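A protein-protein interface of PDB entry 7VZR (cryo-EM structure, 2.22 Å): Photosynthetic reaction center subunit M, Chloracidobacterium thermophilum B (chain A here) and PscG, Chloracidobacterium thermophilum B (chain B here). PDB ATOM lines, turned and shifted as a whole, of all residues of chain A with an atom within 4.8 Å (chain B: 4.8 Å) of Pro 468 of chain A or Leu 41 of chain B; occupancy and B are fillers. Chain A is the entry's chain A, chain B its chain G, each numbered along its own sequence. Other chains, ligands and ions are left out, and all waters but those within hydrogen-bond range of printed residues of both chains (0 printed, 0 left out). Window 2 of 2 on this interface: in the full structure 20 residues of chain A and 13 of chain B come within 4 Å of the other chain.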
ATOM      1  N   PHE A 466       2.154  12.073   2.598  1.00  0.00           N
ATOM      2  CA  PHE A 466       2.786  11.214   1.584  1.00  0.00           C
ATOM      3  C   PHE A 466       3.505  12.238   0.711  1.00  0.00           C
ATOM      4  O   PHE A 466       2.834  13.091   0.129  1.00  0.00           O
ATOM      5  CB  PHE A 466       1.774  10.361   0.826  1.00  0.00           C
ATOM      6  CG  PHE A 466       2.449   9.320  -0.031  1.00  0.00           C
ATOM      7  CD1 PHE A 466       2.790   8.089   0.492  1.00  0.00           C
ATOM      8  CD2 PHE A 466       2.794   9.598  -1.344  1.00  0.00           C
ATOM      9  CE1 PHE A 466       3.437   7.143  -0.287  1.00  0.00           C
ATOM     10  CE2 PHE A 466       3.444   8.655  -2.123  1.00  0.00           C
ATOM     11  CZ  PHE A 466       3.765   7.429  -1.591  1.00  0.00           C
ATOM     12  N   ARG A 467       4.807  12.147   0.572  1.00  0.00           N
ATOM     13  CA  ARG A 467       5.647  13.123  -0.039  1.00  0.00           C
ATOM     14  C   ARG A 467       6.403  12.475  -1.167  1.00  0.00           C
ATOM     15  O   ARG A 467       7.075  11.486  -0.931  1.00  0.00           O
ATOM     16  CB  ARG A 467       6.615  13.680   0.974  1.00  0.00           C
ATOM     17  CG  ARG A 467       7.719  14.532   0.433  1.00  0.00           C
ATOM     18  CD  ARG A 467       7.592  15.836   1.006  1.00  0.00           C
ATOM     19  NE  ARG A 467       8.248  15.991   2.274  1.00  0.00           N
ATOM     20  CZ  ARG A 467       7.882  16.840   3.213  1.00  0.00           C
ATOM     21  NH1 ARG A 467       6.813  17.598   3.094  1.00  0.00           N
ATOM     22  NH2 ARG A 467       8.587  16.895   4.297  1.00  0.00           N
ATOM     23  N   PRO A 468       6.300  12.953  -2.387  1.00  0.00           N
ATOM     24  CA  PRO A 468       6.937  12.233  -3.484  1.00  0.00           C
ATOM     25  C   PRO A 468       8.420  12.490  -3.535  1.00  0.00           C
ATOM     26  O   PRO A 468       8.924  13.476  -2.990  1.00  0.00           O
ATOM     27  CB  PRO A 468       6.235  12.793  -4.717  1.00  0.00           C
ATOM     28  CG  PRO A 468       5.025  13.414  -4.211  1.00  0.00           C
ATOM     29  CD  PRO A 468       5.409  13.993  -2.892  1.00  0.00           C
ATOM     30  N   LYS A 469       9.147  11.611  -4.162  1.00  0.00           N
ATOM     31  CA  LYS A 469      10.565  11.764  -4.220  1.00  0.00           C
ATOM     32  C   LYS A 469      11.023  12.811  -5.169  1.00  0.00           C
ATOM     33  O   LYS A 469      11.790  13.662  -4.861  1.00  0.00           O
ATOM     34  CB  LYS A 469      11.178  10.431  -4.601  1.00  0.00           C
ATOM     35  CG  LYS A 469      11.378   9.615  -3.371  1.00  0.00           C
ATOM     36  CD  LYS A 469      11.660   8.140  -3.572  1.00  0.00           C
ATOM     37  CE  LYS A 469      10.430   7.376  -4.047  1.00  0.00           C
ATOM     38  NZ  LYS A 469      10.508   5.939  -3.714  1.00  0.00           N
ATOM     39  N   ASN A 470      10.530  12.744  -6.374  1.00  0.00           N
ATOM     40  CA  ASN A 470      10.971  13.721  -7.360  1.00  0.00           C
ATOM     41  C   ASN A 470       9.923  13.770  -8.357  1.00  0.00           C
ATOM     42  O   ASN A 470       9.904  13.006  -9.232  1.00  0.00           O
ATOM     43  CB  ASN A 470      12.240  13.282  -8.013  1.00  0.00           C
ATOM     44  CG  ASN A 470      12.658  14.161  -9.125  1.00  0.00           C
ATOM     45  OD1 ASN A 470      13.459  13.746  -9.914  1.00  0.00           O
ATOM     46  ND2 ASN A 470      12.125  15.391  -9.196  1.00  0.00           N
ATOM     47  N   PRO A 471       9.002  14.640  -8.168  1.00  0.00           N
ATOM     48  CA  PRO A 471       7.860  14.864  -9.051  1.00  0.00           C
ATOM     49  C   PRO A 471       8.204  14.835 -10.546  1.00  0.00           C
ATOM     50  O   PRO A 471       7.640  14.157 -11.295  1.00  0.00           O
ATOM     51  CB  PRO A 471       7.444  16.281  -8.706  1.00  0.00           C
ATOM     52  CG  PRO A 471       7.942  16.486  -7.307  1.00  0.00           C
ATOM     53  CD  PRO A 471       9.134  15.629  -7.112  1.00  0.00           C
ATOM     54  N   ALA A 476       8.834   7.439 -10.455  1.00  0.00           N
ATOM     55  CA  ALA A 476       8.853   8.294  -9.353  1.00  0.00           C
ATOM     56  C   ALA A 476       8.818   7.525  -8.103  1.00  0.00           C
ATOM     57  O   ALA A 476       9.699   6.812  -7.836  1.00  0.00           O
ATOM     58  CB  ALA A 476       7.641   9.241  -9.478  1.00  0.00           C
ATOM     59  N   GLY A 477       7.758   7.632  -7.351  1.00  0.00           N
ATOM     60  CA  GLY A 477       7.685   6.980  -6.072  1.00  0.00           C
ATOM     61  C   GLY A 477       7.622   8.054  -5.002  1.00  0.00           C
ATOM     62  O   GLY A 477       7.999   9.158  -5.240  1.00  0.00           O
ATOM     63  N   GLY A 478       7.116   7.696  -3.856  1.00  0.00           N
ATOM     64  CA  GLY A 478       6.993   8.560  -2.746  1.00  0.00           C
ATOM     65  C   GLY A 478       6.926   7.754  -1.524  1.00  0.00           C
ATOM     66  O   GLY A 478       6.919   6.563  -1.517  1.00  0.00           O
ATOM     67  N   GLY A 499       3.467  19.628  -3.745  1.00  0.00           N
ATOM     68  CA  GLY A 499       3.527  18.228  -3.986  1.00  0.00           C
ATOM     69  C   GLY A 499       3.077  17.340  -2.846  1.00  0.00           C
ATOM     70  O   GLY A 499       2.887  16.176  -3.088  1.00  0.00           O
ATOM     71  N   ASP A 500       2.961  17.738  -1.634  1.00  0.00           N
ATOM     72  CA  ASP A 500       2.483  16.849  -0.571  1.00  0.00           C
ATOM     73  C   ASP A 500       1.083  16.368  -0.649  1.00  0.00           C
ATOM     74  O   ASP A 500       0.253  17.053  -1.124  1.00  0.00           O
ATOM     75  CB  ASP A 500       2.497  17.548   0.702  1.00  0.00           C
ATOM     76  CG  ASP A 500       3.816  17.884   1.193  1.00  0.00           C
ATOM     77  OD1 ASP A 500       4.832  17.477   0.784  1.00  0.00           O
ATOM     78  OD2 ASP A 500       3.873  18.685   2.041  1.00  0.00           O
ATOM     79  N   ARG A 501       0.782  15.189  -0.189  1.00  0.00           N
ATOM     80  CA  ARG A 501      -0.551  14.718  -0.198  1.00  0.00           C
ATOM     81  C   ARG A 501      -1.059  14.383   1.086  1.00  0.00           C
ATOM     82  O   ARG A 501      -0.470  13.753   1.799  1.00  0.00           O
ATOM     83  CB  ARG A 501      -0.766  13.572  -1.143  1.00  0.00           C
ATOM     84  CG  ARG A 501       0.079  13.580  -2.315  1.00  0.00           C
ATOM     85  CD  ARG A 501      -0.504  13.861  -3.631  1.00  0.00           C
ATOM     86  NE  ARG A 501       0.683  14.333  -4.324  1.00  0.00           N
ATOM     87  CZ  ARG A 501       0.936  14.730  -5.613  1.00  0.00           C
ATOM     88  NH1 ARG A 501       2.170  15.069  -5.862  1.00  0.00           N
ATOM     89  NH2 ARG A 501       0.071  14.766  -6.617  1.00  0.00           N
ATOM     90  N   VAL B  38       1.712   3.474  -8.589  1.00  0.00           N
ATOM     91  CA  VAL B  38       2.436   4.380  -7.692  1.00  0.00           C
ATOM     92  C   VAL B  38       3.638   5.074  -8.265  1.00  0.00           C
ATOM     93  O   VAL B  38       4.579   5.329  -7.588  1.00  0.00           O
ATOM     94  CB  VAL B  38       2.558   3.883  -6.229  1.00  0.00           C
ATOM     95  CG1 VAL B  38       2.681   5.023  -5.254  1.00  0.00           C
ATOM     96  CG2 VAL B  38       1.364   3.045  -5.839  1.00  0.00           C
ATOM     97  N   LYS B  39       3.511   5.473  -9.534  1.00  0.00           N
ATOM     98  CA  LYS B  39       4.568   6.135 -10.327  1.00  0.00           C
ATOM     99  C   LYS B  39       4.078   7.298 -11.085  1.00  0.00           C
ATOM    100  O   LYS B  39       2.901   7.368 -11.269  1.00  0.00           O
ATOM    101  CB  LYS B  39       5.047   5.204 -11.401  1.00  0.00           C
ATOM    102  CG  LYS B  39       6.306   4.480 -11.141  1.00  0.00           C
ATOM    103  CD  LYS B  39       6.080   3.007 -11.272  1.00  0.00           C
ATOM    104  CE  LYS B  39       7.393   2.279 -11.311  1.00  0.00           C
ATOM    105  NZ  LYS B  39       7.963   2.315  -9.928  1.00  0.00           N
ATOM    106  N   MET B  40       4.963   8.156 -11.580  1.00  0.00           N
ATOM    107  CA  MET B  40       4.604   9.331 -12.379  1.00  0.00           C
ATOM    108  C   MET B  40       3.669  10.088 -11.443  1.00  0.00           C
ATOM    109  O   MET B  40       2.544  10.337 -11.683  1.00  0.00           O
ATOM    110  CB  MET B  40       4.094   8.913 -13.804  1.00  0.00           C
ATOM    111  CG  MET B  40       3.760   9.956 -14.837  1.00  0.00           C
ATOM    112  SD  MET B  40       2.291   9.536 -15.805  1.00  0.00           S
ATOM    113  CE  MET B  40       2.563  10.403 -17.337  1.00  0.00           C
ATOM    114  N   LEU B  41       4.255  10.440 -10.312  1.00  0.00           N
ATOM    115  CA  LEU B  41       3.588  11.058  -9.205  1.00  0.00           C
ATOM    116  C   LEU B  41       3.135  12.476  -9.327  1.00  0.00           C
ATOM    117  O   LEU B  41       2.615  12.941  -8.412  1.00  0.00           O
ATOM    118  CB  LEU B  41       4.407  10.878  -7.905  1.00  0.00           C
ATOM    119  CG  LEU B  41       4.103   9.587  -7.166  1.00  0.00           C
ATOM    120  CD1 LEU B  41       4.911   8.527  -7.775  1.00  0.00           C
ATOM    121  CD2 LEU B  41       4.385   9.586  -5.695  1.00  0.00           C
ATOM    122  N   MET B  42       3.330  13.153 -10.432  1.00  0.00           N
ATOM    123  CA  MET B  42       2.853  14.486 -10.668  1.00  0.00           C
ATOM    124  C   MET B  42       1.309  14.547 -10.902  1.00  0.00           C
ATOM    125  O   MET B  42       0.691  15.615 -10.802  1.00  0.00           O
ATOM    126  CB  MET B  42       3.645  15.024 -11.895  1.00  0.00           C
ATOM    127  CG  MET B  42       3.492  16.472 -12.295  1.00  0.00           C
ATOM    128  SD  MET B  42       4.756  17.663 -11.788  1.00  0.00           S
ATOM    129  CE  MET B  42       6.252  17.175 -12.655  1.00  0.00           C
ATOM    130  N   PHE B  43       0.688  13.420 -11.222  1.00  0.00           N
ATOM    131  CA  PHE B  43      -0.718  13.383 -11.539  1.00  0.00           C
ATOM    132  C   PHE B  43      -1.541  12.577 -10.592  1.00  0.00           C
ATOM    133  O   PHE B  43      -2.683  12.287 -10.777  1.00  0.00           O
ATOM    134  CB  PHE B  43      -0.910  12.875 -12.943  1.00  0.00           C
ATOM    135  CG  PHE B  43      -0.414  13.793 -13.964  1.00  0.00           C
ATOM    136  CD1 PHE B  43      -0.841  15.081 -14.003  1.00  0.00           C
ATOM    137  CD2 PHE B  43       0.510  13.380 -14.888  1.00  0.00           C
ATOM    138  CE1 PHE B  43      -0.390  15.921 -14.961  1.00  0.00           C
ATOM    139  CE2 PHE B  43       0.998  14.239 -15.831  1.00  0.00           C
ATOM    140  CZ  PHE B  43       0.536  15.511 -15.880  1.00  0.00           C
ATOM    141  N   LEU B  44      -0.950  12.269  -9.508  1.00  0.00           N
ATOM    142  CA  LEU B  44      -1.613  11.533  -8.511  1.00  0.00           C
ATOM    143  C   LEU B  44      -2.558  12.407  -7.635  1.00  0.00           C
ATOM    144  O   LEU B  44      -2.261  13.532  -7.328  1.00  0.00           O
ATOM    145  CB  LEU B  44      -0.490  11.023  -7.824  1.00  0.00           C
ATOM    146  CG  LEU B  44      -0.310   9.487  -7.760  1.00  0.00           C
ATOM    147  CD1 LEU B  44      -1.392   8.431  -7.535  1.00  0.00           C
ATOM    148  CD2 LEU B  44       0.989   8.910  -8.294  1.00  0.00           C
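Pro 468 of chain A touches one residue of chain B. Of chain A, only Phe 466, Pro 468, Ala 476, Gly 477, Gly 478 and Arg 501 come within 4 Å of Leu 41 of chain B. Printed residues of chain B within 4 Å of Gly 478 of chain A: Leu 41 (3.8 Å). Printed residues of chain B within 4 Å of Arg 501 of chain A: Leu 41 and Leu 44. The nearest printed residue of chain B that does not touch Pro 468 of chain A is Met 42 of chain B (6.4 Å). The nearest printed residue of chain A that does not touch Leu 41 of chain B is Pro 471 of chain A (5.1 Å). The nearest printed residue of chain A that does not touch Lys 39 of chain B is Gly 477 of chain A (4.6 Å).
Phe 466 of chain A touches Leu 41 of chain B. Leu 41 of chain B touches Pro 468 of chain A (CD2 to CB, 3.8 Å). Pro 471 of chain A touches Met 42 of chain B. Lys 39 of chain B touches Ala 476 of chain A. CB of Ala 476 of chain A touches N of Met 40 of chain B (3.6 Å). Ala 476 of chain A touches Leu 41 of chain B. Val 38 of chain B touches Gly 477 of chain A. CD1 of Leu 41 of chain B touches N of Gly 477 of chain A, at 3.0 Å. Gly 478 of chain A touches Leu 41 of chain B (N to CD2, 3.8 Å).
The guanidinium group of Arg 501 of chain A sits at hydrogen-bond distance from the backbone carbonyl oxygen of Leu 44 of chain B (2.7 Å). NH1 of Arg 501 of chain A is in hydrogen-bond range of O of Leu 41 of chain B, at 3.4 Å.
N of Arg 501 of chain A sits at hydrogen-bond distance from O of Phe 466 of chain A, 3.0 Å away. The backbone carbonyl oxygen (O) of Gly 477 of chain A sits at hydrogen-bond distance from the backbone NH (N) of Lys 469 of chain A, 2.9 Å away. The backbone carbonyl oxygen (O) of Gly 499 of chain A is in hydrogen-bond range of the guanidinium group (NH1) of Arg 501 of chain A (3.1 Å).
Along chain B the printed residues that touch a printed residue of chain A span positions 38 to 44. Of the 12 printed residues of chain A, 7 touch a printed residue of chain B. Hydrophobic or aromatic side chains of chain A within 4 Å of the printed part of chain B: Phe 466, Pro 468 and Ala 476.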
